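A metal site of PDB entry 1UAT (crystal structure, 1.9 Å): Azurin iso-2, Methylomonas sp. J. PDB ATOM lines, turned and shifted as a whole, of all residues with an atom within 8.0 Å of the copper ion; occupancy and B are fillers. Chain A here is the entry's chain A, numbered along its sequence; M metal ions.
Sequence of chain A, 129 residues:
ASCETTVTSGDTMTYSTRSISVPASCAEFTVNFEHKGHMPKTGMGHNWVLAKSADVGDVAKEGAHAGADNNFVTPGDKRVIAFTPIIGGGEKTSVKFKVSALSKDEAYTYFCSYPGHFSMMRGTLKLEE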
ATOM      1  N   SER A   9      13.074 -11.963   2.548  1.00  0.00           N
ATOM      2  CA  SER A   9      11.837 -11.406   3.074  1.00  0.00           C
ATOM      3  C   SER A   9      10.842 -11.270   1.927  1.00  0.00           C
ATOM      4  O   SER A   9      11.171 -11.505   0.760  1.00  0.00           O
ATOM      5  CB  SER A   9      12.084 -10.026   3.698  1.00  0.00           C
ATOM      6  OG  SER A   9      12.464  -9.079   2.719  1.00  0.00           O
ATOM      7  N   GLY A  10       9.610 -10.895   2.255  1.00  0.00           N
ATOM      8  CA  GLY A  10       8.610 -10.679   1.216  1.00  0.00           C
ATOM      9  C   GLY A  10       7.476  -9.816   1.778  1.00  0.00           C
ATOM     10  O   GLY A  10       7.712  -8.979   2.648  1.00  0.00           O
ATOM     11  N   THR A  12       5.288 -10.162   4.017  1.00  0.00           N
ATOM     12  CA  THR A  12       4.948 -10.706   5.317  1.00  0.00           C
ATOM     13  C   THR A  12       5.880 -10.057   6.350  1.00  0.00           C
ATOM     14  O   THR A  12       6.787  -9.334   5.947  1.00  0.00           O
ATOM     15  CB  THR A  12       5.145 -12.226   5.445  1.00  0.00           C
ATOM     16  OG1 THR A  12       6.545 -12.522   5.393  1.00  0.00           O
ATOM     17  CG2 THR A  12       4.442 -13.058   4.382  1.00  0.00           C
ATOM     18  N   MET A  13       5.706 -10.354   7.628  1.00  0.00           N
ATOM     19  CA  MET A  13       6.538  -9.754   8.665  1.00  0.00           C
ATOM     20  C   MET A  13       7.585 -10.725   9.195  1.00  0.00           C
ATOM     21  O   MET A  13       7.944 -10.698  10.372  1.00  0.00           O
ATOM     22  CB  MET A  13       5.659  -9.213   9.788  1.00  0.00           C
ATOM     23  CG  MET A  13       4.801  -8.030   9.383  1.00  0.00           C
ATOM     24  SD  MET A  13       5.750  -6.610   8.797  1.00  0.00           S
ATOM     25  CE  MET A  13       4.892  -6.231   7.265  1.00  0.00           C
ATOM     26  N   THR A  14       8.054 -11.652   8.360  1.00  0.00           N
ATOM     27  CA  THR A  14       8.952 -12.718   8.763  1.00  0.00           C
ATOM     28  C   THR A  14      10.180 -12.820   7.864  1.00  0.00           C
ATOM     29  O   THR A  14      10.105 -12.618   6.648  1.00  0.00           O
ATOM     30  CB  THR A  14       8.236 -14.082   8.724  1.00  0.00           C
ATOM     31  OG1 THR A  14       6.957 -13.994   9.365  1.00  0.00           O
ATOM     32  CG2 THR A  14       9.045 -15.149   9.453  1.00  0.00           C
ATOM     33  N   TYR A  15      11.332 -13.111   8.458  1.00  0.00           N
ATOM     34  CA  TYR A  15      12.541 -13.400   7.696  1.00  0.00           C
ATOM     35  C   TYR A  15      12.476 -14.873   7.295  1.00  0.00           C
ATOM     36  O   TYR A  15      11.840 -15.650   8.011  1.00  0.00           O
ATOM     37  CB  TYR A  15      13.799 -13.166   8.524  1.00  0.00           C
ATOM     38  CG  TYR A  15      14.195 -11.723   8.767  1.00  0.00           C
ATOM     39  CD1 TYR A  15      14.531 -10.886   7.720  1.00  0.00           C
ATOM     40  CD2 TYR A  15      14.234 -11.220  10.057  1.00  0.00           C
ATOM     41  CE1 TYR A  15      14.919  -9.579   7.951  1.00  0.00           C
ATOM     42  CE2 TYR A  15      14.636  -9.928  10.313  1.00  0.00           C
ATOM     43  CZ  TYR A  15      14.963  -9.115   9.248  1.00  0.00           C
ATOM     44  OH  TYR A  15      15.375  -7.822   9.468  1.00  0.00           O
ATOM     45  N   PHE A  33      20.723  -9.805   1.468  1.00  0.00           N
ATOM     46  CA  PHE A  33      19.336  -9.653   1.899  1.00  0.00           C
ATOM     47  C   PHE A  33      18.449  -9.389   0.693  1.00  0.00           C
ATOM     48  O   PHE A  33      18.748  -8.486  -0.080  1.00  0.00           O
ATOM     49  CB  PHE A  33      19.217  -8.527   2.932  1.00  0.00           C
ATOM     50  CG  PHE A  33      17.815  -8.303   3.429  1.00  0.00           C
ATOM     51  CD1 PHE A  33      17.215  -7.064   3.306  1.00  0.00           C
ATOM     52  CD2 PHE A  33      17.120  -9.320   4.069  1.00  0.00           C
ATOM     53  CE1 PHE A  33      15.931  -6.851   3.777  1.00  0.00           C
ATOM     54  CE2 PHE A  33      15.842  -9.106   4.553  1.00  0.00           C
ATOM     55  CZ  PHE A  33      15.251  -7.871   4.402  1.00  0.00           C
ATOM     56  N   HIS A  35      14.450  -9.057  -1.095  1.00  0.00           N
ATOM     57  CA  HIS A  35      13.019  -8.832  -0.883  1.00  0.00           C
ATOM     58  C   HIS A  35      12.268  -9.477  -2.043  1.00  0.00           C
ATOM     59  O   HIS A  35      12.364  -9.012  -3.182  1.00  0.00           O
ATOM     60  CB  HIS A  35      12.701  -7.346  -0.747  1.00  0.00           C
ATOM     61  CG  HIS A  35      11.322  -7.031  -0.258  1.00  0.00           C
ATOM     62  ND1 HIS A  35      10.190  -7.691  -0.708  1.00  0.00           N
ATOM     63  CD2 HIS A  35      10.905  -6.091   0.622  1.00  0.00           C
ATOM     64  CE1 HIS A  35       9.144  -7.171  -0.092  1.00  0.00           C
ATOM     65  NE2 HIS A  35       9.538  -6.193   0.703  1.00  0.00           N
ATOM     66  N   GLY A  43       4.091  -0.005   3.492  1.00  0.00           N
ATOM     67  CA  GLY A  43       4.321  -0.704   4.746  1.00  0.00           C
ATOM     68  C   GLY A  43       5.121  -1.997   4.612  1.00  0.00           C
ATOM     69  O   GLY A  43       5.286  -2.708   5.599  1.00  0.00           O
ATOM     70  N   MET A  44       5.597  -2.293   3.409  1.00  0.00           N
ATOM     71  CA  MET A  44       6.286  -3.553   3.153  1.00  0.00           C
ATOM     72  C   MET A  44       7.762  -3.384   2.820  1.00  0.00           C
ATOM     73  O   MET A  44       8.361  -4.338   2.308  1.00  0.00           O
ATOM     74  CB  MET A  44       5.574  -4.357   2.062  1.00  0.00           C
ATOM     75  CG  MET A  44       4.220  -4.934   2.413  1.00  0.00           C
ATOM     76  SD  MET A  44       4.146  -6.146   3.747  1.00  0.00           S
ATOM     77  CE  MET A  44       5.837  -6.706   3.875  1.00  0.00           C
ATOM     78  N   GLY A  45       8.375  -2.274   3.197  1.00  0.00           N
ATOM     79  CA  GLY A  45       9.824  -2.106   3.050  1.00  0.00           C
ATOM     80  C   GLY A  45      10.521  -2.817   4.205  1.00  0.00           C
ATOM     81  O   GLY A  45       9.953  -2.965   5.295  1.00  0.00           O
ATOM     82  N   HIS A  46      11.675  -3.426   3.943  1.00  0.00           N
ATOM     83  CA  HIS A  46      12.378  -4.169   4.987  1.00  0.00           C
ATOM     84  C   HIS A  46      13.874  -3.886   4.937  1.00  0.00           C
ATOM     85  O   HIS A  46      14.432  -3.629   3.878  1.00  0.00           O
ATOM     86  CB  HIS A  46      12.176  -5.679   4.875  1.00  0.00           C
ATOM     87  CG  HIS A  46      10.804  -6.254   4.881  1.00  0.00           C
ATOM     88  ND1 HIS A  46       9.939  -6.124   5.949  1.00  0.00           N
ATOM     89  CD2 HIS A  46      10.133  -6.972   3.938  1.00  0.00           C
ATOM     90  CE1 HIS A  46       8.804  -6.752   5.672  1.00  0.00           C
ATOM     91  NE2 HIS A  46       8.905  -7.271   4.466  1.00  0.00           N
ATOM     92  N   ASN A  47      14.527  -4.043   6.092  1.00  0.00           N
ATOM     93  CA  ASN A  47      15.987  -4.052   6.138  1.00  0.00           C
ATOM     94  C   ASN A  47      16.435  -5.129   7.119  1.00  0.00           C
ATOM     95  O   ASN A  47      15.615  -5.871   7.655  1.00  0.00           O
ATOM     96  CB  ASN A  47      16.558  -2.679   6.474  1.00  0.00           C
ATOM     97  CG  ASN A  47      16.206  -2.146   7.847  1.00  0.00           C
ATOM     98  OD1 ASN A  47      15.458  -2.765   8.609  1.00  0.00           O
ATOM     99  ND2 ASN A  47      16.707  -0.958   8.148  1.00  0.00           N
ATOM    100  N   TRP A  48      17.740  -5.199   7.336  1.00  0.00           N
ATOM    101  CA  TRP A  48      18.348  -6.124   8.287  1.00  0.00           C
ATOM    102  C   TRP A  48      19.355  -5.349   9.137  1.00  0.00           C
ATOM    103  O   TRP A  48      20.233  -4.663   8.607  1.00  0.00           O
ATOM    104  CB  TRP A  48      19.068  -7.249   7.546  1.00  0.00           C
ATOM    105  CG  TRP A  48      19.689  -8.345   8.358  1.00  0.00           C
ATOM    106  CD1 TRP A  48      19.136  -9.563   8.634  1.00  0.00           C
ATOM    107  CD2 TRP A  48      21.009  -8.389   8.905  1.00  0.00           C
ATOM    108  NE1 TRP A  48      19.995 -10.331   9.370  1.00  0.00           N
ATOM    109  CE2 TRP A  48      21.165  -9.637   9.533  1.00  0.00           C
ATOM    110  CE3 TRP A  48      22.063  -7.477   8.947  1.00  0.00           C
ATOM    111  CZ2 TRP A  48      22.327  -9.998  10.211  1.00  0.00           C
ATOM    112  CZ3 TRP A  48      23.227  -7.843   9.608  1.00  0.00           C
ATOM    113  CH2 TRP A  48      23.355  -9.089  10.226  1.00  0.00           C
ATOM    114  N   ILE A  86      16.868   0.082   3.578  1.00  0.00           N
ATOM    115  CA  ILE A  86      15.514  -0.416   3.391  1.00  0.00           C
ATOM    116  C   ILE A  86      15.361  -0.781   1.921  1.00  0.00           C
ATOM    117  O   ILE A  86      15.698   0.047   1.079  1.00  0.00           O
ATOM    118  CB  ILE A  86      14.460   0.650   3.738  1.00  0.00           C
ATOM    119  CG1 ILE A  86      14.443   0.931   5.239  1.00  0.00           C
ATOM    120  CG2 ILE A  86      13.067   0.273   3.257  1.00  0.00           C
ATOM    121  CD1 ILE A  86      13.886  -0.140   6.145  1.00  0.00           C
ATOM    122  N   ILE A  87      14.831  -1.963   1.626  1.00  0.00           N
ATOM    123  CA  ILE A  87      14.579  -2.326   0.235  1.00  0.00           C
ATOM    124  C   ILE A  87      13.096  -2.692   0.088  1.00  0.00           C
ATOM    125  O   ILE A  87      12.443  -3.084   1.050  1.00  0.00           O
ATOM    126  CB  ILE A  87      15.451  -3.504  -0.239  1.00  0.00           C
ATOM    127  CG1 ILE A  87      15.394  -4.661   0.761  1.00  0.00           C
ATOM    128  CG2 ILE A  87      16.897  -3.078  -0.469  1.00  0.00           C
ATOM    129  CD1 ILE A  87      15.845  -5.974   0.151  1.00  0.00           C
ATOM    130  N   PHE A 111      17.039  -7.542  13.225  1.00  0.00           N
ATOM    131  CA  PHE A 111      15.646  -7.138  13.158  1.00  0.00           C
ATOM    132  C   PHE A 111      15.441  -6.099  12.054  1.00  0.00           C
ATOM    133  O   PHE A 111      16.407  -5.592  11.477  1.00  0.00           O
ATOM    134  CB  PHE A 111      15.182  -6.493  14.469  1.00  0.00           C
ATOM    135  CG  PHE A 111      15.973  -5.281  14.865  1.00  0.00           C
ATOM    136  CD1 PHE A 111      17.218  -5.430  15.461  1.00  0.00           C
ATOM    137  CD2 PHE A 111      15.504  -3.997  14.621  1.00  0.00           C
ATOM    138  CE1 PHE A 111      17.978  -4.327  15.815  1.00  0.00           C
ATOM    139  CE2 PHE A 111      16.250  -2.896  14.974  1.00  0.00           C
ATOM    140  CZ  PHE A 111      17.491  -3.063  15.557  1.00  0.00           C
ATOM    141  N   CYS A 112      14.180  -5.869  11.705  1.00  0.00           N
ATOM    142  CA  CYS A 112      13.852  -4.867  10.702  1.00  0.00           C
ATOM    143  C   CYS A 112      13.447  -3.567  11.401  1.00  0.00           C
ATOM    144  O   CYS A 112      12.604  -3.653  12.297  1.00  0.00           O
ATOM    145  CB  CYS A 112      12.664  -5.395   9.879  1.00  0.00           C
ATOM    146  SG  CYS A 112      12.123  -4.193   8.645  1.00  0.00           S
ATOM    147  N   SER A 113      14.038  -2.430  11.064  1.00  0.00           N
ATOM    148  CA  SER A 113      13.692  -1.185  11.745  1.00  0.00           C
ATOM    149  C   SER A 113      12.656  -0.338  11.011  1.00  0.00           C
ATOM    150  O   SER A 113      12.313   0.748  11.487  1.00  0.00           O
ATOM    151  CB  SER A 113      14.965  -0.379  12.024  1.00  0.00           C
ATOM    152  OG  SER A 113      15.478   0.125  10.801  1.00  0.00           O
ATOM    153  N   TYR A 114      12.047  -0.811   9.923  1.00  0.00           N
ATOM    154  CA  TYR A 114      10.882  -0.143   9.347  1.00  0.00           C
ATOM    155  C   TYR A 114       9.812  -0.044  10.437  1.00  0.00           C
ATOM    156  O   TYR A 114       9.646  -0.980  11.219  1.00  0.00           O
ATOM    157  CB  TYR A 114      10.354  -0.918   8.135  1.00  0.00           C
ATOM    158  CG  TYR A 114       9.343  -0.182   7.293  1.00  0.00           C
ATOM    159  CD1 TYR A 114       8.030  -0.037   7.704  1.00  0.00           C
ATOM    160  CD2 TYR A 114       9.728   0.437   6.109  1.00  0.00           C
ATOM    161  CE1 TYR A 114       7.096   0.633   6.923  1.00  0.00           C
ATOM    162  CE2 TYR A 114       8.819   1.128   5.331  1.00  0.00           C
ATOM    163  CZ  TYR A 114       7.514   1.216   5.749  1.00  0.00           C
ATOM    164  OH  TYR A 114       6.605   1.908   4.970  1.00  0.00           O
ATOM    165  N   PRO A 115       9.207   1.119  10.619  1.00  0.00           N
ATOM    166  CA  PRO A 115       8.362   1.414  11.771  1.00  0.00           C
ATOM    167  C   PRO A 115       7.374   0.301  12.101  1.00  0.00           C
ATOM    168  O   PRO A 115       6.601  -0.101  11.245  1.00  0.00           O
ATOM    169  CB  PRO A 115       7.653   2.706  11.367  1.00  0.00           C
ATOM    170  CG  PRO A 115       8.675   3.400  10.541  1.00  0.00           C
ATOM    171  CD  PRO A 115       9.449   2.341   9.809  1.00  0.00           C
ATOM    172  N   GLY A 116       7.499  -0.244  13.311  1.00  0.00           N
ATOM    173  CA  GLY A 116       6.603  -1.299  13.743  1.00  0.00           C
ATOM    174  C   GLY A 116       7.048  -2.722  13.424  1.00  0.00           C
ATOM    175  O   GLY A 116       6.614  -3.615  14.160  1.00  0.00           O
ATOM    176  N   HIS A 117       7.987  -2.954  12.514  1.00  0.00           N
ATOM    177  CA  HIS A 117       8.308  -4.331  12.135  1.00  0.00           C
ATOM    178  C   HIS A 117       9.171  -5.068  13.142  1.00  0.00           C
ATOM    179  O   HIS A 117       9.138  -6.299  13.192  1.00  0.00           O
ATOM    180  CB  HIS A 117       9.015  -4.362  10.784  1.00  0.00           C
ATOM    181  CG  HIS A 117       8.197  -3.896   9.613  1.00  0.00           C
ATOM    182  ND1 HIS A 117       8.606  -4.130   8.321  1.00  0.00           N
ATOM    183  CD2 HIS A 117       6.974  -3.321   9.517  1.00  0.00           C
ATOM    184  CE1 HIS A 117       7.716  -3.633   7.473  1.00  0.00           C
ATOM    185  NE2 HIS A 117       6.724  -3.130   8.174  1.00  0.00           N
ATOM    186  N   PHE A 118       9.931  -4.364  13.972  1.00  0.00           N
ATOM    187  CA  PHE A 118      10.929  -4.968  14.837  1.00  0.00           C
ATOM    188  C   PHE A 118      10.362  -5.937  15.868  1.00  0.00           C
ATOM    189  O   PHE A 118      11.101  -6.789  16.359  1.00  0.00           O
ATOM    190  CB  PHE A 118      11.782  -3.880  15.500  1.00  0.00           C
ATOM    191  CG  PHE A 118      11.187  -3.287  16.751  1.00  0.00           C
ATOM    192  CD1 PHE A 118      10.320  -2.211  16.678  1.00  0.00           C
ATOM    193  CD2 PHE A 118      11.520  -3.797  17.993  1.00  0.00           C
ATOM    194  CE1 PHE A 118       9.790  -1.660  17.823  1.00  0.00           C
ATOM    195  CE2 PHE A 118      10.970  -3.260  19.140  1.00  0.00           C
ATOM    196  CZ  PHE A 118      10.110  -2.182  19.055  1.00  0.00           C
ATOM    197  N   MET A 121       9.528  -9.086  13.287  1.00  0.00           N
ATOM    198  CA  MET A 121      10.569  -9.389  12.308  1.00  0.00           C
ATOM    199  C   MET A 121      11.954  -9.372  12.922  1.00  0.00           C
ATOM    200  O   MET A 121      12.610  -8.338  12.968  1.00  0.00           O
ATOM    201  CB  MET A 121      10.455  -8.366  11.178  1.00  0.00           C
ATOM    202  CG  MET A 121      10.995  -8.895   9.863  1.00  0.00           C
ATOM    203  SD  MET A 121      10.347  -7.997   8.445  1.00  0.00           S
ATOM    204  CE  MET A 121      11.378  -8.712   7.164  1.00  0.00           C
HETATM  205 CU    CU M   1      10.355  -5.072   7.743  1.00  0.00          CU
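OH of Tyr 15 is in hydrogen-bond range of N of Cys 112 (3.2 Å).
A ring nitrogen (ND1) of His 46 lies close to the side-chain sulfur (SD) of Met 121 (3.1 Å).
The backbone NH (N) of Ile 87 is in hydrogen-bond range of the backbone carbonyl oxygen (O) of His 46 (2.8 Å).
N of Cys 112 sits at hydrogen-bond distance from O of Met 121.
A ring nitrogen (NE2) of His 46 lies close to the backbone carbonyl oxygen of Thr 12, at 3.3 Å.
A ring nitrogen (NE2) of His 117 sits close to the side-chain sulfur (SD) of Met 13, at 3.7 Å.
The backbone carbonyl oxygen (O) of Gly 43 sits at hydrogen-bond distance from a ring nitrogen (NE2) of His 117, at 3.0 Å.
NE2 of His 46 is in hydrogen-bond range of O of Gly 10.
Residues that only touch the copper ion: Gly 45 (3.3 Å).
Along chain A the residues within 4 Å of the copper ion span positions 45 to 121.
ND1 of His 117 is bound to the copper ion (2.1 Å).
The copper ion is bound by a ring nitrogen (ND1) of His 46 (2.1 Å).
The side-chain sulfur (SG) of Cys 112 is bound to the copper ion (2.2 Å).
Slightly farther from the copper ion lies SD of Met 121 (3.0 Å).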
